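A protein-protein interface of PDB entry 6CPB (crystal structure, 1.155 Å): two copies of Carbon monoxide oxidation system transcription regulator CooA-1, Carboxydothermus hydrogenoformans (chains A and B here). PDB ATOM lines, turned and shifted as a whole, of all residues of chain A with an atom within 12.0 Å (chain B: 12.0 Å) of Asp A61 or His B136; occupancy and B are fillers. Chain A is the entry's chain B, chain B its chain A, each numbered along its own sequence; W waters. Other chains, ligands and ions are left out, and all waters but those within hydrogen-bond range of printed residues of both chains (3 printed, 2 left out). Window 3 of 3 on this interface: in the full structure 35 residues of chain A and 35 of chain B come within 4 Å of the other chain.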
ATOM      1  N   TYR A  56      -9.963  16.996 -26.317  1.00  0.00           N
ATOM      2  CA  TYR A  56      -9.977  18.422 -26.001  1.00  0.00           C
ATOM      3  C   TYR A  56      -8.720  18.851 -25.250  1.00  0.00           C
ATOM      4  O   TYR A  56      -7.961  18.035 -24.721  1.00  0.00           O
ATOM      5  CB  TYR A  56     -11.232  18.774 -25.189  1.00  0.00           C
ATOM      6  CG  TYR A  56     -11.270  18.189 -23.798  1.00  0.00           C
ATOM      7  CD1 TYR A  56     -11.547  16.849 -23.599  1.00  0.00           C
ATOM      8  CD2 TYR A  56     -11.009  18.978 -22.679  1.00  0.00           C
ATOM      9  CE1 TYR A  56     -11.579  16.308 -22.337  1.00  0.00           C
ATOM     10  CE2 TYR A  56     -11.047  18.452 -21.404  1.00  0.00           C
ATOM     11  CZ  TYR A  56     -11.326  17.108 -21.236  1.00  0.00           C
ATOM     12  OH  TYR A  56     -11.384  16.525 -19.982  1.00  0.00           O
ATOM     13  N   LEU A  57      -8.536  20.171 -25.207  1.00  0.00           N
ATOM     14  CA  LEU A  57      -7.520  20.852 -24.404  1.00  0.00           C
ATOM     15  C   LEU A  57      -8.244  21.947 -23.641  1.00  0.00           C
ATOM     16  O   LEU A  57      -8.808  22.853 -24.256  1.00  0.00           O
ATOM     17  CB  LEU A  57      -6.449  21.488 -25.291  1.00  0.00           C
ATOM     18  CG  LEU A  57      -5.669  20.572 -26.216  1.00  0.00           C
ATOM     19  CD1 LEU A  57      -4.880  21.418 -27.234  1.00  0.00           C
ATOM     20  CD2 LEU A  57      -4.741  19.664 -25.437  1.00  0.00           C
ATOM     21  N   ALA A  58      -8.235  21.871 -22.314  1.00  0.00           N
ATOM     22  CA  ALA A  58      -8.961  22.822 -21.483  1.00  0.00           C
ATOM     23  C   ALA A  58      -8.010  23.577 -20.567  1.00  0.00           C
ATOM     24  O   ALA A  58      -7.213  22.973 -19.838  1.00  0.00           O
ATOM     25  CB  ALA A  58     -10.021  22.112 -20.651  1.00  0.00           C
ATOM     26  N   TYR A  59      -8.110  24.902 -20.592  1.00  0.00           N
ATOM     27  CA  TYR A  59      -7.276  25.789 -19.790  1.00  0.00           C
ATOM     28  C   TYR A  59      -8.168  26.712 -18.971  1.00  0.00           C
ATOM     29  O   TYR A  59      -9.369  26.845 -19.217  1.00  0.00           O
ATOM     30  CB  TYR A  59      -6.347  26.621 -20.681  1.00  0.00           C
ATOM     31  CG  TYR A  59      -5.520  25.777 -21.610  1.00  0.00           C
ATOM     32  CD1 TYR A  59      -4.297  25.284 -21.220  1.00  0.00           C
ATOM     33  CD2 TYR A  59      -5.984  25.458 -22.879  1.00  0.00           C
ATOM     34  CE1 TYR A  59      -3.541  24.490 -22.074  1.00  0.00           C
ATOM     35  CE2 TYR A  59      -5.243  24.677 -23.732  1.00  0.00           C
ATOM     36  CZ  TYR A  59      -4.026  24.194 -23.329  1.00  0.00           C
ATOM     37  OH  TYR A  59      -3.313  23.407 -24.201  1.00  0.00           O
ATOM     38  N   GLU A  60      -7.561  27.395 -17.997  1.00  0.00           N
ATOM     39  CA  GLU A  60      -8.340  28.303 -17.161  1.00  0.00           C
ATOM     40  C   GLU A  60      -9.086  29.314 -18.022  1.00  0.00           C
ATOM     41  O   GLU A  60     -10.230  29.676 -17.724  1.00  0.00           O
ATOM     42  CB  GLU A  60      -7.427  29.032 -16.177  1.00  0.00           C
ATOM     43  CG  GLU A  60      -8.215  29.824 -15.145  1.00  0.00           C
ATOM     44  CD  GLU A  60      -7.344  30.596 -14.192  1.00  0.00           C
ATOM     45  OE1 GLU A  60      -6.258  31.027 -14.616  1.00  0.00           O
ATOM     46  OE2 GLU A  60      -7.749  30.779 -13.022  1.00  0.00           O
ATOM     47  N   ASP A  61      -8.436  29.780 -19.084  1.00  0.00           N
ATOM     48  CA  ASP A  61      -8.870  30.931 -19.859  1.00  0.00           C
ATOM     49  C   ASP A  61      -9.411  30.580 -21.235  1.00  0.00           C
ATOM     50  O   ASP A  61      -9.827  31.492 -21.953  1.00  0.00           O
ATOM     51  CB  ASP A  61      -7.734  31.980 -19.970  1.00  0.00           C
ATOM     52  CG  ASP A  61      -6.367  31.380 -20.339  1.00  0.00           C
ATOM     53  OD1 ASP A  61      -6.102  30.202 -20.007  1.00  0.00           O
ATOM     54  OD2 ASP A  61      -5.539  32.123 -20.937  1.00  0.00           O
ATOM     55  N   LYS A  62      -9.441  29.303 -21.610  1.00  0.00           N
ATOM     56  CA  LYS A  62      -9.756  28.949 -22.989  1.00  0.00           C
ATOM     57  C   LYS A  62      -9.908  27.441 -23.091  1.00  0.00           C
ATOM     58  O   LYS A  62      -9.214  26.704 -22.400  1.00  0.00           O
ATOM     59  CB  LYS A  62      -8.602  29.397 -23.887  1.00  0.00           C
ATOM     60  CG  LYS A  62      -8.960  29.552 -25.329  1.00  0.00           C
ATOM     61  CD  LYS A  62      -7.981  30.507 -26.032  1.00  0.00           C
ATOM     62  CE  LYS A  62      -8.288  31.981 -25.759  1.00  0.00           C
ATOM     63  NZ  LYS A  62      -7.311  32.904 -26.401  1.00  0.00           N
ATOM     64  N   GLU A  63     -10.800  26.987 -23.974  1.00  0.00           N
ATOM     65  CA  GLU A  63     -10.976  25.566 -24.243  1.00  0.00           C
ATOM     66  C   GLU A  63     -10.999  25.334 -25.747  1.00  0.00           C
ATOM     67  O   GLU A  63     -11.481  26.170 -26.515  1.00  0.00           O
ATOM     68  CB  GLU A  63     -12.287  25.036 -23.614  1.00  0.00           C
ATOM     69  CG  GLU A  63     -12.358  23.519 -23.518  1.00  0.00           C
ATOM     70  CD  GLU A  63     -13.685  23.023 -22.975  1.00  0.00           C
ATOM     71  OE1 GLU A  63     -13.742  22.618 -21.788  1.00  0.00           O
ATOM     72  OE2 GLU A  63     -14.669  23.022 -23.747  1.00  0.00           O
ATOM     73  N   PHE A  64     -10.499  24.167 -26.154  1.00  0.00           N
ATOM     74  CA  PHE A  64     -10.525  23.730 -27.543  1.00  0.00           C
ATOM     75  C   PHE A  64     -11.065  22.315 -27.603  1.00  0.00           C
ATOM     76  O   PHE A  64     -10.520  21.417 -26.963  1.00  0.00           O
ATOM     77  CB  PHE A  64      -9.120  23.740 -28.160  1.00  0.00           C
ATOM     78  CG  PHE A  64      -8.409  25.047 -27.993  1.00  0.00           C
ATOM     79  CD1 PHE A  64      -8.563  26.064 -28.914  1.00  0.00           C
ATOM     80  CD2 PHE A  64      -7.614  25.269 -26.887  1.00  0.00           C
ATOM     81  CE1 PHE A  64      -7.910  27.272 -28.742  1.00  0.00           C
ATOM     82  CE2 PHE A  64      -6.961  26.473 -26.715  1.00  0.00           C
ATOM     83  CZ  PHE A  64      -7.103  27.465 -27.644  1.00  0.00           C
ATOM     84  N   THR A  65     -12.106  22.109 -28.392  1.00  0.00           N
ATOM     85  CA  THR A  65     -12.623  20.771 -28.650  1.00  0.00           C
ATOM     86  C   THR A  65     -12.107  20.344 -30.014  1.00  0.00           C
ATOM     87  O   THR A  65     -12.493  20.905 -31.043  1.00  0.00           O
ATOM     88  CB  THR A  65     -14.145  20.733 -28.584  1.00  0.00           C
ATOM     89  OG1 THR A  65     -14.573  21.105 -27.270  1.00  0.00           O
ATOM     90  CG2 THR A  65     -14.673  19.325 -28.874  1.00  0.00           C
ATOM     91  N   ILE A 127      -7.069  26.052 -35.627  1.00  0.00           N
ATOM     92  CA  ILE A 127      -7.002  26.611 -34.282  1.00  0.00           C
ATOM     93  C   ILE A 127      -5.758  27.470 -34.134  1.00  0.00           C
ATOM     94  O   ILE A 127      -5.816  28.585 -33.607  1.00  0.00           O
ATOM     95  CB  ILE A 127      -7.042  25.489 -33.227  1.00  0.00           C
ATOM     96  CG1 ILE A 127      -8.418  24.824 -33.204  1.00  0.00           C
ATOM     97  CG2 ILE A 127      -6.658  26.039 -31.845  1.00  0.00           C
ATOM     98  CD1 ILE A 127      -8.472  23.565 -32.367  1.00  0.00           C
ATOM     99  N   LEU A 131      -5.517  31.547 -33.218  1.00  0.00           N
ATOM    100  CA  LEU A 131      -4.757  32.132 -32.124  1.00  0.00           C
ATOM    101  C   LEU A 131      -3.784  33.182 -32.641  1.00  0.00           C
ATOM    102  O   LEU A 131      -3.655  34.267 -32.052  1.00  0.00           O
ATOM    103  CB  LEU A 131      -4.014  31.036 -31.363  1.00  0.00           C
ATOM    104  CG  LEU A 131      -4.910  30.049 -30.611  1.00  0.00           C
ATOM    105  CD1 LEU A 131      -4.097  28.908 -30.052  1.00  0.00           C
ATOM    106  CD2 LEU A 131      -5.714  30.729 -29.494  1.00  0.00           C
ATOM    107  N   VAL A 132      -3.100  32.884 -33.747  1.00  0.00           N
ATOM    108  CA  VAL A 132      -2.175  33.850 -34.330  1.00  0.00           C
ATOM    109  C   VAL A 132      -2.911  35.116 -34.732  1.00  0.00           C
ATOM    110  O   VAL A 132      -2.439  36.230 -34.480  1.00  0.00           O
ATOM    111  CB  VAL A 132      -1.447  33.220 -35.529  1.00  0.00           C
ATOM    112  CG1 VAL A 132      -0.668  34.270 -36.301  1.00  0.00           C
ATOM    113  CG2 VAL A 132      -0.521  32.107 -35.069  1.00  0.00           C
ATOM    114  N   LEU A 134      -5.560  36.531 -33.482  1.00  0.00           N
ATOM    115  CA  LEU A 134      -5.921  37.416 -32.381  1.00  0.00           C
ATOM    116  C   LEU A 134      -4.693  38.006 -31.704  1.00  0.00           C
ATOM    117  O   LEU A 134      -4.748  39.134 -31.205  1.00  0.00           O
ATOM    118  CB  LEU A 134      -6.825  36.683 -31.400  1.00  0.00           C
ATOM    119  CG  LEU A 134      -8.199  36.334 -31.987  1.00  0.00           C
ATOM    120  CD1 LEU A 134      -8.959  35.465 -31.021  1.00  0.00           C
ATOM    121  CD2 LEU A 134      -9.027  37.574 -32.326  1.00  0.00           C
ATOM    122  N   GLU A 135      -3.586  37.270 -31.682  1.00  0.00           N
ATOM    123  CA  GLU A 135      -2.333  37.797 -31.154  1.00  0.00           C
ATOM    124  C   GLU A 135      -1.852  38.950 -32.017  1.00  0.00           C
ATOM    125  O   GLU A 135      -1.455  40.009 -31.516  1.00  0.00           O
ATOM    126  CB  GLU A 135      -1.298  36.671 -31.197  1.00  0.00           C
ATOM    127  CG  GLU A 135      -0.253  36.672 -30.114  1.00  0.00           C
ATOM    128  CD  GLU A 135       0.924  35.773 -30.469  1.00  0.00           C
ATOM    129  OE1 GLU A 135       1.892  36.269 -31.088  1.00  0.00           O
ATOM    130  OE2 GLU A 135       0.870  34.564 -30.151  1.00  0.00           O
ATOM    131  N   HIS A 136      -1.902  38.752 -33.336  1.00  0.00           N
ATOM    132  CA  HIS A 136      -1.353  39.717 -34.279  1.00  0.00           C
ATOM    133  C   HIS A 136      -2.204  40.977 -34.363  1.00  0.00           C
ATOM    134  O   HIS A 136      -1.686  42.048 -34.695  1.00  0.00           O
ATOM    135  CB  HIS A 136      -1.262  39.054 -35.653  1.00  0.00           C
ATOM    136  CG  HIS A 136      -0.581  39.897 -36.684  1.00  0.00           C
ATOM    137  ND1 HIS A 136       0.613  40.544 -36.446  1.00  0.00           N
ATOM    138  CD2 HIS A 136      -0.921  40.192 -37.961  1.00  0.00           C
ATOM    139  CE1 HIS A 136       0.977  41.204 -37.531  1.00  0.00           C
ATOM    140  NE2 HIS A 136       0.064  41.005 -38.466  1.00  0.00           N
ATOM    141  N   HIS A 138      -3.907  42.268 -31.757  1.00  0.00           N
ATOM    142  CA  HIS A 138      -4.057  42.884 -30.440  1.00  0.00           C
ATOM    143  C   HIS A 138      -3.241  44.170 -30.352  1.00  0.00           C
ATOM    144  O   HIS A 138      -2.192  44.299 -30.985  1.00  0.00           O
ATOM    145  CB  HIS A 138      -3.622  41.916 -29.338  1.00  0.00           C
ATOM    146  N   ILE B 127       2.076  23.044 -30.243  1.00  0.00           N
ATOM    147  CA  ILE B 127       2.086  24.458 -30.617  1.00  0.00           C
ATOM    148  C   ILE B 127       0.919  25.194 -29.970  1.00  0.00           C
ATOM    149  O   ILE B 127       1.097  26.287 -29.418  1.00  0.00           O
ATOM    150  CB  ILE B 127       2.100  24.621 -32.148  1.00  0.00           C
ATOM    151  CG1 ILE B 127       3.422  24.115 -32.718  1.00  0.00           C
ATOM    152  CG2 ILE B 127       1.847  26.079 -32.554  1.00  0.00           C
ATOM    153  CD1 ILE B 127       3.352  23.740 -34.188  1.00  0.00           C
ATOM    154  N   ILE B 128      -0.287  24.614 -30.027  1.00  0.00           N
ATOM    155  CA  ILE B 128      -1.439  25.249 -29.392  1.00  0.00           C
ATOM    156  C   ILE B 128      -1.167  25.472 -27.910  1.00  0.00           C
ATOM    157  O   ILE B 128      -1.397  26.561 -27.369  1.00  0.00           O
ATOM    158  CB  ILE B 128      -2.704  24.399 -29.605  1.00  0.00           C
ATOM    159  CG1 ILE B 128      -3.114  24.400 -31.080  1.00  0.00           C
ATOM    160  CG2 ILE B 128      -3.845  24.919 -28.728  1.00  0.00           C
ATOM    161  CD1 ILE B 128      -4.150  23.347 -31.427  1.00  0.00           C
ATOM    162  N   ASN B 129      -0.679  24.434 -27.236  1.00  0.00           N
ATOM    163  CA  ASN B 129      -0.417  24.510 -25.807  1.00  0.00           C
ATOM    164  C   ASN B 129       0.567  25.634 -25.494  1.00  0.00           C
ATOM    165  O   ASN B 129       0.414  26.356 -24.499  1.00  0.00           O
ATOM    166  CB  ASN B 129       0.112  23.147 -25.345  1.00  0.00           C
ATOM    167  CG  ASN B 129       0.149  23.006 -23.845  1.00  0.00           C
ATOM    168  OD1 ASN B 129      -0.886  22.964 -23.192  1.00  0.00           O
ATOM    169  ND2 ASN B 129       1.344  22.937 -23.291  1.00  0.00           N
ATOM    170  N   GLY B 130       1.580  25.805 -26.342  1.00  0.00           N
ATOM    171  CA  GLY B 130       2.544  26.873 -26.133  1.00  0.00           C
ATOM    172  C   GLY B 130       1.969  28.252 -26.383  1.00  0.00           C
ATOM    173  O   GLY B 130       2.209  29.175 -25.604  1.00  0.00           O
ATOM    174  N   LEU B 131       1.190  28.409 -27.455  1.00  0.00           N
ATOM    175  CA  LEU B 131       0.589  29.704 -27.743  1.00  0.00           C
ATOM    176  C   LEU B 131      -0.352  30.142 -26.626  1.00  0.00           C
ATOM    177  O   LEU B 131      -0.390  31.328 -26.267  1.00  0.00           O
ATOM    178  CB  LEU B 131      -0.154  29.666 -29.080  1.00  0.00           C
ATOM    179  CG  LEU B 131       0.728  29.570 -30.322  1.00  0.00           C
ATOM    180  CD1 LEU B 131      -0.143  29.344 -31.550  1.00  0.00           C
ATOM    181  CD2 LEU B 131       1.585  30.809 -30.495  1.00  0.00           C
ATOM    182  N   VAL B 132      -1.130  29.210 -26.075  1.00  0.00           N
ATOM    183  CA  VAL B 132      -2.043  29.568 -24.996  1.00  0.00           C
ATOM    184  C   VAL B 132      -1.262  30.124 -23.810  1.00  0.00           C
ATOM    185  O   VAL B 132      -1.642  31.142 -23.215  1.00  0.00           O
ATOM    186  CB  VAL B 132      -2.915  28.360 -24.596  1.00  0.00           C
ATOM    187  CG1 VAL B 132      -3.729  28.680 -23.346  1.00  0.00           C
ATOM    188  CG2 VAL B 132      -3.833  27.979 -25.722  1.00  0.00           C
ATOM    189  N   PHE B 133      -0.162  29.467 -23.444  1.00  0.00           N
ATOM    190  CA  PHE B 133       0.639  29.971 -22.337  1.00  0.00           C
ATOM    191  C   PHE B 133       1.237  31.339 -22.659  1.00  0.00           C
ATOM    192  O   PHE B 133       1.174  32.271 -21.848  1.00  0.00           O
ATOM    193  CB  PHE B 133       1.743  28.980 -21.979  1.00  0.00           C
ATOM    194  CG  PHE B 133       2.585  29.444 -20.824  1.00  0.00           C
ATOM    195  CD1 PHE B 133       2.056  29.487 -19.553  1.00  0.00           C
ATOM    196  CD2 PHE B 133       3.891  29.879 -21.014  1.00  0.00           C
ATOM    197  CE1 PHE B 133       2.821  29.955 -18.479  1.00  0.00           C
ATOM    198  CE2 PHE B 133       4.659  30.335 -19.949  1.00  0.00           C
ATOM    199  CZ  PHE B 133       4.121  30.353 -18.689  1.00  0.00           C
ATOM    200  N   LEU B 134       1.815  31.485 -23.847  1.00  0.00           N
ATOM    201  CA  LEU B 134       2.522  32.714 -24.183  1.00  0.00           C
ATOM    202  C   LEU B 134       1.581  33.893 -24.330  1.00  0.00           C
ATOM    203  O   LEU B 134       2.015  35.038 -24.161  1.00  0.00           O
ATOM    204  CB  LEU B 134       3.274  32.531 -25.500  1.00  0.00           C
ATOM    205  CG  LEU B 134       4.415  31.520 -25.478  1.00  0.00           C
ATOM    206  CD1 LEU B 134       4.870  31.217 -26.898  1.00  0.00           C
ATOM    207  CD2 LEU B 134       5.569  31.999 -24.629  1.00  0.00           C
ATOM    208  N   GLU B 135       0.308  33.643 -24.627  1.00  0.00           N
ATOM    209  CA  GLU B 135      -0.667  34.699 -24.807  1.00  0.00           C
ATOM    210  C   GLU B 135      -1.452  34.997 -23.542  1.00  0.00           C
ATOM    211  O   GLU B 135      -2.222  35.960 -23.527  1.00  0.00           O
ATOM    212  CB  GLU B 135      -1.650  34.304 -25.920  1.00  0.00           C
ATOM    213  CG  GLU B 135      -0.996  34.125 -27.297  1.00  0.00           C
ATOM    214  CD  GLU B 135      -1.913  33.488 -28.339  1.00  0.00           C
ATOM    215  OE1 GLU B 135      -2.992  32.979 -27.965  1.00  0.00           O
ATOM    216  OE2 GLU B 135      -1.546  33.495 -29.537  1.00  0.00           O
ATOM    217  N   HIS B 136      -1.276  34.217 -22.479  1.00  0.00           N
ATOM    218  CA  HIS B 136      -2.159  34.349 -21.332  1.00  0.00           C
ATOM    219  C   HIS B 136      -1.856  35.625 -20.561  1.00  0.00           C
ATOM    220  O   HIS B 136      -0.728  36.123 -20.554  1.00  0.00           O
ATOM    221  CB  HIS B 136      -2.105  33.100 -20.434  1.00  0.00           C
ATOM    222  CG  HIS B 136      -1.152  33.166 -19.272  1.00  0.00           C
ATOM    223  ND1 HIS B 136       0.172  32.787 -19.363  1.00  0.00           N
ATOM    224  CD2 HIS B 136      -1.365  33.459 -17.965  1.00  0.00           C
ATOM    225  CE1 HIS B 136       0.742  32.873 -18.172  1.00  0.00           C
ATOM    226  NE2 HIS B 136      -0.166  33.294 -17.307  1.00  0.00           N
ATOM    227  N   HIS B 137      -2.897  36.166 -19.934  1.00  0.00           N
ATOM    228  CA  HIS B 137      -2.786  37.360 -19.117  1.00  0.00           C
ATOM    229  C   HIS B 137      -3.790  37.247 -17.984  1.00  0.00           C
ATOM    230  O   HIS B 137      -4.798  36.543 -18.091  1.00  0.00           O
ATOM    231  CB  HIS B 137      -3.080  38.629 -19.926  1.00  0.00           C
ATOM    232  CG  HIS B 137      -2.095  38.894 -21.020  1.00  0.00           C
ATOM    233  ND1 HIS B 137      -2.433  38.833 -22.356  1.00  0.00           N
ATOM    234  CD2 HIS B 137      -0.781  39.219 -20.980  1.00  0.00           C
ATOM    235  CE1 HIS B 137      -1.371  39.111 -23.089  1.00  0.00           C
ATOM    236  NE2 HIS B 137      -0.355  39.348 -22.280  1.00  0.00           N
ATOM    237  N   HIS B 138      -3.513  37.960 -16.896  1.00  0.00           N
ATOM    238  CA  HIS B 138      -4.377  37.920 -15.719  1.00  0.00           C
ATOM    239  C   HIS B 138      -5.737  38.535 -16.032  1.00  0.00           C
ATOM    240  O   HIS B 138      -5.820  39.574 -16.686  1.00  0.00           O
ATOM    241  CB  HIS B 138      -3.725  38.665 -14.554  1.00  0.00           C
HETATM  242  O   HOH W   1      -4.720  32.290 -26.088  1.00  0.00           O
HETATM  243  O   HOH W   2      -5.564  34.812 -20.718  1.00  0.00           O
HETATM  244  O   HOH W   3      -4.078  32.383 -23.407  1.00  0.00           O
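CD1 of Leu A57 touches CG2 of Ile B128, 3.9 Å away. Tyr A59 touches Val B132. OD2 of Asp A61 touches CB of His B136, 3.6 Å away. Phe A64 touches Val B132 (CE2 to CG2, 3.6 Å). Ile A127 touches Ile B128 (CG2 to CD1, 3.7 Å). Glu A135 touches Leu B131.
The side-chain hydroxyl (OH) of Tyr A59 sits at hydrogen-bond distance from the side-chain amide oxygen (OD1) of Asn B129 (2.7 Å). OE2 of Glu B135 lies close to OE2 of Glu A135, at 2.7 Å. The side-chain carboxylate (OE2) of Glu B135 lies close to the backbone carbonyl oxygen (O) of Leu A131 (3.4 Å).
Leu A131 touches Glu B135, and with the chains exchanged Glu A135 touches Leu B131. Glu A135 touches its own counterpart, Glu B135. 7 positions are printed for both chains.
Hydrophobic or aromatic side chains of chain B that line the printed part of chain A: Ile B128, Leu B131, Val B132 and His B136. Printed residues of chain A that touch a printed residue of chain B: Leu A57, Tyr A59, Asp A61, Phe A64, Ile A127, Leu A131 and Glu A135. Hydrophobic or aromatic side chains of chain A that line the printed part of chain B: Leu A57, Tyr A59, Phe A64, Ile A127 and Leu A131. Among the printed residues, 9 pairs touch across the chains. Among the printed residues, no Asp or Glu carboxylate lies within 4 Å of a Lys or Arg side-chain nitrogen of the other chain.
Asp A61 touches just one residue of chain B: His B136 (3.6 Å). No residue of chain B comes within 4 Å of Glu A60. No residue of chain B comes within 4 Å of Lys A62. No residue of chain A comes within 4 Å of Phe B133. No residue of chain A comes within 4 Å of His B137. No residue of chain A comes within 4 Å of His B138. Of the printed residues of chain A, Ile B128 touches Leu A57 and Ile A127. Of the printed residues of chain B, Leu A57 touches Ile B128 (3.9 Å). Printed residues of chain B within 4 Å of Leu A131: Glu B135. Tyr A56 touches none of the printed residues of chain B. The nearest printed residue of chain B that does not touch Tyr A59 is Ile B128 (4.8 Å).
The backbone carbonyl oxygen of Phe B133 sits at hydrogen-bond distance from a ring nitrogen (ND1) of His B136. The backbone carbonyl oxygen (O) of Glu B135 sits at hydrogen-bond distance from a ring nitrogen (ND1) of His B137 (3.1 Å). The backbone carbonyl oxygen of Leu A57 lies within hydrogen-bond range of the backbone NH of Phe A64 (2.9 Å).
Water W1 bridges OE1 of Glu B135 (2.6 Å) and NZ of Lys A62 (2.7 Å). Water W2 bridges OD2 of Asp A61 (2.7 Å) and N of His B137 (3.1 Å). Water W3 lies within hydrogen-bond range of O of Val B132 (2.7 Å), OD2 of Asp A61 (2.9 Å) and N of His B136 (3.5 Å).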
